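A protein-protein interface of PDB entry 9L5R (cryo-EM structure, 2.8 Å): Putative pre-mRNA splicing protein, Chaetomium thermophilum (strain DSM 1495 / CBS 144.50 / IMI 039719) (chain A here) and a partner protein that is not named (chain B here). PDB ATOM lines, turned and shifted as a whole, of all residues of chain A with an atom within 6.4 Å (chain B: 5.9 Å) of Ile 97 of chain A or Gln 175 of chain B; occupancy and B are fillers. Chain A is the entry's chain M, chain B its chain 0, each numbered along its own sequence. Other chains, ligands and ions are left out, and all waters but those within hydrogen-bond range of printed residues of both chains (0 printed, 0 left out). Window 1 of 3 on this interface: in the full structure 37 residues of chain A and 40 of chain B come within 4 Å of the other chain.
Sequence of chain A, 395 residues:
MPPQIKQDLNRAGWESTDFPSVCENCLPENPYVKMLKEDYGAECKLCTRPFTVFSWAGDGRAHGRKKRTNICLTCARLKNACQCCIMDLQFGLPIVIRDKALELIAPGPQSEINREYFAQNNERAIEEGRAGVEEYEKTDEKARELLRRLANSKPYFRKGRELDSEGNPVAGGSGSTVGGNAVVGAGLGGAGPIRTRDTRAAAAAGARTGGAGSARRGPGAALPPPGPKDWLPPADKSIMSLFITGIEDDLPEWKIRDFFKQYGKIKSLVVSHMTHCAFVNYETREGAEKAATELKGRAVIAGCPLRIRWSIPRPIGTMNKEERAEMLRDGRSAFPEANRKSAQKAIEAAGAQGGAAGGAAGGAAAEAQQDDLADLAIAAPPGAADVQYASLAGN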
ATOM      1  N   LEU A  93       3.129   5.769 -17.949  1.00  0.00           N
ATOM      2  CA  LEU A  93       1.829   5.686 -17.338  1.00  0.00           C
ATOM      3  C   LEU A  93       1.882   6.264 -15.934  1.00  0.00           C
ATOM      4  O   LEU A  93       2.950   6.300 -15.323  1.00  0.00           O
ATOM      5  CB  LEU A  93       1.356   4.232 -17.258  1.00  0.00           C
ATOM      6  CG  LEU A  93       0.914   3.528 -18.537  1.00  0.00           C
ATOM      7  CD1 LEU A  93       0.778   2.043 -18.285  1.00  0.00           C
ATOM      8  CD2 LEU A  93      -0.391   4.111 -19.024  1.00  0.00           C
ATOM      9  N   PRO A  94       0.758   6.736 -15.402  1.00  0.00           N
ATOM     10  CA  PRO A  94       0.670   6.939 -13.956  1.00  0.00           C
ATOM     11  C   PRO A  94       0.929   5.629 -13.231  1.00  0.00           C
ATOM     12  O   PRO A  94       0.613   4.551 -13.733  1.00  0.00           O
ATOM     13  CB  PRO A  94      -0.767   7.420 -13.754  1.00  0.00           C
ATOM     14  CG  PRO A  94      -1.117   8.056 -15.033  1.00  0.00           C
ATOM     15  CD  PRO A  94      -0.397   7.307 -16.109  1.00  0.00           C
ATOM     16  N   ILE A  95       1.561   5.737 -12.061  1.00  0.00           N
ATOM     17  CA  ILE A  95       2.009   4.555 -11.331  1.00  0.00           C
ATOM     18  C   ILE A  95       0.823   3.686 -10.942  1.00  0.00           C
ATOM     19  O   ILE A  95       0.883   2.453 -11.029  1.00  0.00           O
ATOM     20  CB  ILE A  95       2.842   4.983 -10.108  1.00  0.00           C
ATOM     21  CG1 ILE A  95       4.210   5.473 -10.561  1.00  0.00           C
ATOM     22  CG2 ILE A  95       3.007   3.855  -9.109  1.00  0.00           C
ATOM     23  CD1 ILE A  95       4.958   4.465 -11.361  1.00  0.00           C
ATOM     24  N   VAL A  96      -0.292   4.316 -10.572  1.00  0.00           N
ATOM     25  CA  VAL A  96      -1.480   3.563 -10.189  1.00  0.00           C
ATOM     26  C   VAL A  96      -2.076   2.840 -11.396  1.00  0.00           C
ATOM     27  O   VAL A  96      -2.515   1.694 -11.280  1.00  0.00           O
ATOM     28  CB  VAL A  96      -2.495   4.486  -9.481  1.00  0.00           C
ATOM     29  CG1 VAL A  96      -2.954   5.644 -10.377  1.00  0.00           C
ATOM     30  CG2 VAL A  96      -3.676   3.689  -8.958  1.00  0.00           C
ATOM     31  N   ILE A  97      -2.050   3.461 -12.579  1.00  0.00           N
ATOM     32  CA  ILE A  97      -2.575   2.808 -13.778  1.00  0.00           C
ATOM     33  C   ILE A  97      -1.685   1.647 -14.194  1.00  0.00           C
ATOM     34  O   ILE A  97      -2.179   0.556 -14.514  1.00  0.00           O
ATOM     35  CB  ILE A  97      -2.739   3.825 -14.919  1.00  0.00           C
ATOM     36  CG1 ILE A  97      -3.703   4.937 -14.517  1.00  0.00           C
ATOM     37  CG2 ILE A  97      -3.223   3.141 -16.169  1.00  0.00           C
ATOM     38  CD1 ILE A  97      -4.996   4.451 -13.929  1.00  0.00           C
ATOM     39  N   ARG A  98      -0.364   1.860 -14.179  1.00  0.00           N
ATOM     40  CA  ARG A  98       0.588   0.802 -14.504  1.00  0.00           C
ATOM     41  C   ARG A  98       0.395  -0.391 -13.583  1.00  0.00           C
ATOM     42  O   ARG A  98       0.279  -1.530 -14.043  1.00  0.00           O
ATOM     43  CB  ARG A  98       2.022   1.336 -14.388  1.00  0.00           C
ATOM     44  CG  ARG A  98       3.176   0.426 -14.892  1.00  0.00           C
ATOM     45  CD  ARG A  98       3.685  -0.609 -13.882  1.00  0.00           C
ATOM     46  NE  ARG A  98       4.107  -0.061 -12.597  1.00  0.00           N
ATOM     47  CZ  ARG A  98       5.307   0.437 -12.335  1.00  0.00           C
ATOM     48  NH1 ARG A  98       6.271   0.431 -13.238  1.00  0.00           N
ATOM     49  NH2 ARG A  98       5.556   0.915 -11.123  1.00  0.00           N
ATOM     50  N   ASP A  99       0.341  -0.147 -12.277  1.00  0.00           N
ATOM     51  CA  ASP A  99       0.280  -1.256 -11.341  1.00  0.00           C
ATOM     52  C   ASP A  99      -1.114  -1.853 -11.228  1.00  0.00           C
ATOM     53  O   ASP A  99      -1.240  -3.022 -10.861  1.00  0.00           O
ATOM     54  CB  ASP A  99       0.800  -0.807  -9.978  1.00  0.00           C
ATOM     55  CG  ASP A  99       2.317  -0.711  -9.943  1.00  0.00           C
ATOM     56  OD1 ASP A  99       2.861   0.357 -10.296  1.00  0.00           O
ATOM     57  OD2 ASP A  99       2.971  -1.706  -9.569  1.00  0.00           O
ATOM     58  N   LYS A 100      -2.159  -1.105 -11.579  1.00  0.00           N
ATOM     59  CA  LYS A 100      -3.495  -1.681 -11.600  1.00  0.00           C
ATOM     60  C   LYS A 100      -3.674  -2.600 -12.797  1.00  0.00           C
ATOM     61  O   LYS A 100      -4.243  -3.690 -12.672  1.00  0.00           O
ATOM     62  CB  LYS A 100      -4.537  -0.564 -11.621  1.00  0.00           C
ATOM     63  CG  LYS A 100      -5.919  -1.019 -11.246  1.00  0.00           C
ATOM     64  CD  LYS A 100      -5.938  -1.560  -9.833  1.00  0.00           C
ATOM     65  CE  LYS A 100      -5.780  -0.452  -8.819  1.00  0.00           C
ATOM     66  NZ  LYS A 100      -7.012   0.372  -8.728  1.00  0.00           N
ATOM     67  N   ALA A 101      -3.194  -2.180 -13.969  1.00  0.00           N
ATOM     68  CA  ALA A 101      -3.354  -2.989 -15.167  1.00  0.00           C
ATOM     69  C   ALA A 101      -2.366  -4.152 -15.213  1.00  0.00           C
ATOM     70  O   ALA A 101      -2.726  -5.252 -15.641  1.00  0.00           O
ATOM     71  CB  ALA A 101      -3.208  -2.101 -16.391  1.00  0.00           C
ATOM     72  N   LEU A 102      -1.134  -3.943 -14.753  1.00  0.00           N
ATOM     73  CA  LEU A 102      -0.113  -4.978 -14.668  1.00  0.00           C
ATOM     74  C   LEU A 102       0.160  -5.245 -13.203  1.00  0.00           C
ATOM     75  O   LEU A 102       1.322  -5.242 -12.786  1.00  0.00           O
ATOM     76  CB  LEU A 102       1.193  -4.560 -15.341  1.00  0.00           C
ATOM     77  CG  LEU A 102       1.240  -3.976 -16.742  1.00  0.00           C
ATOM     78  CD1 LEU A 102       2.582  -3.334 -16.999  1.00  0.00           C
ATOM     79  CD2 LEU A 102       1.048  -5.109 -17.670  1.00  0.00           C
ATOM     80  N   TYR B 162      -6.599  11.762  -0.356  1.00  0.00           N
ATOM     81  CA  TYR B 162      -7.696  12.698  -0.479  1.00  0.00           C
ATOM     82  C   TYR B 162      -7.887  13.400   0.854  1.00  0.00           C
ATOM     83  O   TYR B 162      -7.494  12.895   1.908  1.00  0.00           O
ATOM     84  CB  TYR B 162      -8.987  11.986  -0.888  1.00  0.00           C
ATOM     85  CG  TYR B 162      -9.114  11.750  -2.371  1.00  0.00           C
ATOM     86  CD1 TYR B 162      -9.449  12.781  -3.230  1.00  0.00           C
ATOM     87  CD2 TYR B 162      -8.898  10.494  -2.911  1.00  0.00           C
ATOM     88  CE1 TYR B 162      -9.564  12.569  -4.575  1.00  0.00           C
ATOM     89  CE2 TYR B 162      -9.010  10.273  -4.255  1.00  0.00           C
ATOM     90  CZ  TYR B 162      -9.344  11.314  -5.083  1.00  0.00           C
ATOM     91  OH  TYR B 162      -9.456  11.101  -6.431  1.00  0.00           O
ATOM     92  N   SER B 171      -5.923  13.519  -5.983  1.00  0.00           N
ATOM     93  CA  SER B 171      -4.910  12.524  -5.683  1.00  0.00           C
ATOM     94  C   SER B 171      -4.312  11.964  -6.963  1.00  0.00           C
ATOM     95  O   SER B 171      -5.032  11.728  -7.936  1.00  0.00           O
ATOM     96  CB  SER B 171      -5.493  11.383  -4.858  1.00  0.00           C
ATOM     97  OG  SER B 171      -4.606  10.283  -4.825  1.00  0.00           O
ATOM     98  N   PHE B 172      -2.999  11.750  -6.964  1.00  0.00           N
ATOM     99  CA  PHE B 172      -2.378  11.022  -8.060  1.00  0.00           C
ATOM    100  C   PHE B 172      -2.424   9.515  -7.859  1.00  0.00           C
ATOM    101  O   PHE B 172      -2.005   8.771  -8.750  1.00  0.00           O
ATOM    102  CB  PHE B 172      -0.927  11.489  -8.302  1.00  0.00           C
ATOM    103  CG  PHE B 172      -0.060  11.564  -7.069  1.00  0.00           C
ATOM    104  CD1 PHE B 172       0.384  10.422  -6.429  1.00  0.00           C
ATOM    105  CD2 PHE B 172       0.363  12.791  -6.595  1.00  0.00           C
ATOM    106  CE1 PHE B 172       1.184  10.501  -5.315  1.00  0.00           C
ATOM    107  CE2 PHE B 172       1.176  12.876  -5.480  1.00  0.00           C
ATOM    108  CZ  PHE B 172       1.586  11.730  -4.841  1.00  0.00           C
ATOM    109  N   ASN B 173      -2.919   9.054  -6.717  1.00  0.00           N
ATOM    110  CA  ASN B 173      -3.131   7.639  -6.465  1.00  0.00           C
ATOM    111  C   ASN B 173      -4.471   7.143  -6.996  1.00  0.00           C
ATOM    112  O   ASN B 173      -4.802   5.972  -6.798  1.00  0.00           O
ATOM    113  CB  ASN B 173      -3.031   7.352  -4.964  1.00  0.00           C
ATOM    114  CG  ASN B 173      -1.601   7.136  -4.500  1.00  0.00           C
ATOM    115  OD1 ASN B 173      -0.690   6.978  -5.307  1.00  0.00           O
ATOM    116  ND2 ASN B 173      -1.402   7.132  -3.190  1.00  0.00           N
ATOM    117  N   ARG B 174      -5.258   8.008  -7.633  1.00  0.00           N
ATOM    118  CA  ARG B 174      -6.480   7.597  -8.319  1.00  0.00           C
ATOM    119  C   ARG B 174      -6.776   8.614  -9.407  1.00  0.00           C
ATOM    120  O   ARG B 174      -6.895   9.807  -9.118  1.00  0.00           O
ATOM    121  CB  ARG B 174      -7.654   7.486  -7.351  1.00  0.00           C
ATOM    122  CG  ARG B 174      -8.671   6.424  -7.736  1.00  0.00           C
ATOM    123  CD  ARG B 174      -9.838   6.382  -6.769  1.00  0.00           C
ATOM    124  NE  ARG B 174     -10.827   7.412  -7.054  1.00  0.00           N
ATOM    125  CZ  ARG B 174     -11.626   7.952  -6.146  1.00  0.00           C
ATOM    126  NH1 ARG B 174     -11.605   7.554  -4.885  1.00  0.00           N
ATOM    127  NH2 ARG B 174     -12.459   8.921  -6.506  1.00  0.00           N
ATOM    128  N   GLN B 175      -6.895   8.148 -10.651  1.00  0.00           N
ATOM    129  CA  GLN B 175      -7.124   9.024 -11.802  1.00  0.00           C
ATOM    130  C   GLN B 175      -8.615   9.324 -11.892  1.00  0.00           C
ATOM    131  O   GLN B 175      -9.349   8.785 -12.722  1.00  0.00           O
ATOM    132  CB  GLN B 175      -6.600   8.378 -13.078  1.00  0.00           C
ATOM    133  CG  GLN B 175      -6.507   9.321 -14.265  1.00  0.00           C
ATOM    134  CD  GLN B 175      -6.202   8.598 -15.568  1.00  0.00           C
ATOM    135  OE1 GLN B 175      -5.874   7.411 -15.570  1.00  0.00           O
ATOM    136  NE2 GLN B 175      -6.322   9.310 -16.683  1.00  0.00           N
ATOM    137  N   ASN B 176      -9.070  10.214 -11.018  1.00  0.00           N
ATOM    138  CA  ASN B 176     -10.494  10.469 -10.844  1.00  0.00           C
ATOM    139  C   ASN B 176     -10.954  11.559 -11.802  1.00  0.00           C
ATOM    140  O   ASN B 176     -10.402  12.663 -11.806  1.00  0.00           O
ATOM    141  CB  ASN B 176     -10.794  10.867  -9.404  1.00  0.00           C
ATOM    142  CG  ASN B 176     -12.260  10.788  -9.077  1.00  0.00           C
ATOM    143  OD1 ASN B 176     -13.012  10.066  -9.723  1.00  0.00           O
ATOM    144  ND2 ASN B 176     -12.677  11.527  -8.066  1.00  0.00           N
ATOM    145  N   ARG B 177     -11.974  11.249 -12.600  1.00  0.00           N
ATOM    146  CA  ARG B 177     -12.578  12.199 -13.525  1.00  0.00           C
ATOM    147  C   ARG B 177     -14.024  12.499 -13.159  1.00  0.00           C
ATOM    148  O   ARG B 177     -14.762  13.067 -13.968  1.00  0.00           O
ATOM    149  CB  ARG B 177     -12.493  11.669 -14.955  1.00  0.00           C
ATOM    150  CG  ARG B 177     -11.112  11.177 -15.330  1.00  0.00           C
ATOM    151  CD  ARG B 177     -11.147  10.171 -16.464  1.00  0.00           C
ATOM    152  NE  ARG B 177     -12.200   9.179 -16.292  1.00  0.00           N
ATOM    153  CZ  ARG B 177     -12.912   8.672 -17.288  1.00  0.00           C
ATOM    154  NH1 ARG B 177     -12.706   9.038 -18.541  1.00  0.00           N
ATOM    155  NH2 ARG B 177     -13.856   7.776 -17.020  1.00  0.00           N
ATOM    156  N   GLU B 223      -9.390  14.677 -17.034  1.00  0.00           N
ATOM    157  CA  GLU B 223      -9.205  15.005 -15.626  1.00  0.00           C
ATOM    158  C   GLU B 223      -9.064  16.504 -15.416  1.00  0.00           C
ATOM    159  O   GLU B 223      -9.529  17.032 -14.401  1.00  0.00           O
ATOM    160  CB  GLU B 223      -7.982  14.272 -15.084  1.00  0.00           C
ATOM    161  CG  GLU B 223      -8.015  14.028 -13.599  1.00  0.00           C
ATOM    162  CD  GLU B 223      -6.929  13.080 -13.150  1.00  0.00           C
ATOM    163  OE1 GLU B 223      -6.066  12.728 -13.978  1.00  0.00           O
ATOM    164  OE2 GLU B 223      -6.938  12.682 -11.968  1.00  0.00           O
ATOM    165  N   GLU B 261     -14.441   0.909 -15.368  1.00  0.00           N
ATOM    166  CA  GLU B 261     -13.245   1.631 -14.953  1.00  0.00           C
ATOM    167  C   GLU B 261     -12.005   0.762 -15.099  1.00  0.00           C
ATOM    168  O   GLU B 261     -10.966   1.230 -15.580  1.00  0.00           O
ATOM    169  CB  GLU B 261     -13.402   2.119 -13.513  1.00  0.00           C
ATOM    170  CG  GLU B 261     -12.199   2.868 -12.950  1.00  0.00           C
ATOM    171  CD  GLU B 261     -11.887   4.161 -13.687  1.00  0.00           C
ATOM    172  OE1 GLU B 261     -12.821   4.801 -14.217  1.00  0.00           O
ATOM    173  OE2 GLU B 261     -10.702   4.549 -13.724  1.00  0.00           O
ATOM    174  N   ARG B 264     -11.196   0.504 -18.752  1.00  0.00           N
ATOM    175  CA  ARG B 264     -10.541   1.723 -19.212  1.00  0.00           C
ATOM    176  C   ARG B 264      -9.087   1.784 -18.758  1.00  0.00           C
ATOM    177  O   ARG B 264      -8.233   2.295 -19.492  1.00  0.00           O
ATOM    178  CB  ARG B 264     -11.317   2.939 -18.718  1.00  0.00           C
ATOM    179  CG  ARG B 264     -10.894   4.239 -19.348  1.00  0.00           C
ATOM    180  CD  ARG B 264     -11.482   5.403 -18.589  1.00  0.00           C
ATOM    181  NE  ARG B 264     -11.062   5.409 -17.194  1.00  0.00           N
ATOM    182  CZ  ARG B 264      -9.928   5.942 -16.762  1.00  0.00           C
ATOM    183  NH1 ARG B 264      -9.067   6.498 -17.594  1.00  0.00           N
ATOM    184  NH2 ARG B 264      -9.655   5.917 -15.460  1.00  0.00           N
ATOM    185  N   ILE B 265      -8.788   1.260 -17.564  1.00  0.00           N
ATOM    186  CA  ILE B 265      -7.402   1.187 -17.093  1.00  0.00           C
ATOM    187  C   ILE B 265      -6.558   0.311 -18.011  1.00  0.00           C
ATOM    188  O   ILE B 265      -5.481   0.722 -18.466  1.00  0.00           O
ATOM    189  CB  ILE B 265      -7.347   0.690 -15.637  1.00  0.00           C
ATOM    190  CG1 ILE B 265      -7.864   1.760 -14.682  1.00  0.00           C
ATOM    191  CG2 ILE B 265      -5.949   0.248 -15.261  1.00  0.00           C
ATOM    192  CD1 ILE B 265      -8.022   1.266 -13.272  1.00  0.00           C
ATOM    193  N   GLN B 268      -6.105   2.126 -21.506  1.00  0.00           N
ATOM    194  CA  GLN B 268      -5.062   3.146 -21.468  1.00  0.00           C
ATOM    195  C   GLN B 268      -3.676   2.518 -21.382  1.00  0.00           C
ATOM    196  O   GLN B 268      -2.750   2.920 -22.108  1.00  0.00           O
ATOM    197  CB  GLN B 268      -5.301   4.081 -20.287  1.00  0.00           C
ATOM    198  CG  GLN B 268      -4.118   4.955 -19.943  1.00  0.00           C
ATOM    199  CD  GLN B 268      -4.457   6.025 -18.931  1.00  0.00           C
ATOM    200  OE1 GLN B 268      -5.466   5.939 -18.232  1.00  0.00           O
ATOM    201  NE2 GLN B 268      -3.616   7.047 -18.851  1.00  0.00           N
ATOM    202  N   ALA B 269      -3.523   1.505 -20.523  1.00  0.00           N
ATOM    203  CA  ALA B 269      -2.228   0.858 -20.371  1.00  0.00           C
ATOM    204  C   ALA B 269      -1.803   0.150 -21.645  1.00  0.00           C
ATOM    205  O   ALA B 269      -0.652   0.272 -22.058  1.00  0.00           O
ATOM    206  CB  ALA B 269      -2.260  -0.125 -19.213  1.00  0.00           C
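The backbone NH (N) of Asn 173 of chain B sits at hydrogen-bond distance from the side-chain hydroxyl (OG) of Ser 171 of chain B, at 2.8 Å. The side-chain amide oxygen (OE1) of Gln 268 of chain B lies close to the side-chain amide oxygen (OE1) of Gln 175 of chain B (3.1 Å).
Among the printed residues, merely in contact across the chains: Val 96 of chain A with Asn 173 of chain B, Ile 97 of chain A with Gln 175 of chain B, Ala 101 of chain A with Ala 269 of chain B, Val 96 of chain A with Phe 172 of chain B, Lys 100 of chain A with Ile 265 of chain B, Ala 101 of chain A with Ile 265 of chain B, Leu 93 of chain A with Ala 269 of chain B, Ile 97 of chain A with Ile 265 of chain B and Leu 93 of chain A with Gln 268 of chain B.
Of chain A, only Ile 97 comes within 4 Å of Gln 175 of chain B. Of the printed residues of chain B, Lys 100 of chain A touches Ile 265 (3.7 Å). Of the printed residues of chain A, Ile 265 of chain B touches Ile 97 (3.9 Å), Lys 100 (3.7 Å) and Ala 101 (3.8 Å). Of the printed residues of chain A, Asn 173 of chain B touches Val 96 (3.3 Å). Asn 176 of chain B touches none of the printed residues of chain A. The nearest residue of chain A that does not touch Gln 175 of chain B is Val 96 of chain A (4.7 Å).
Of the 14 printed residues of chain B, 6 touch a printed residue of chain A. Printed residues of chain B that touch a printed residue of chain A: Phe 172, Asn 173, Gln 175, Ile 265, Gln 268 and Ala 269. Hydrophobic or aromatic side chains of chain B within 4 Å of the printed part of chain A: Ile 265 and Ala 269. Hydrophobic or aromatic side chains of chain A within 4 Å of the printed part of chain B: Leu 93, Val 96, Ile 97 and Ala 101.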
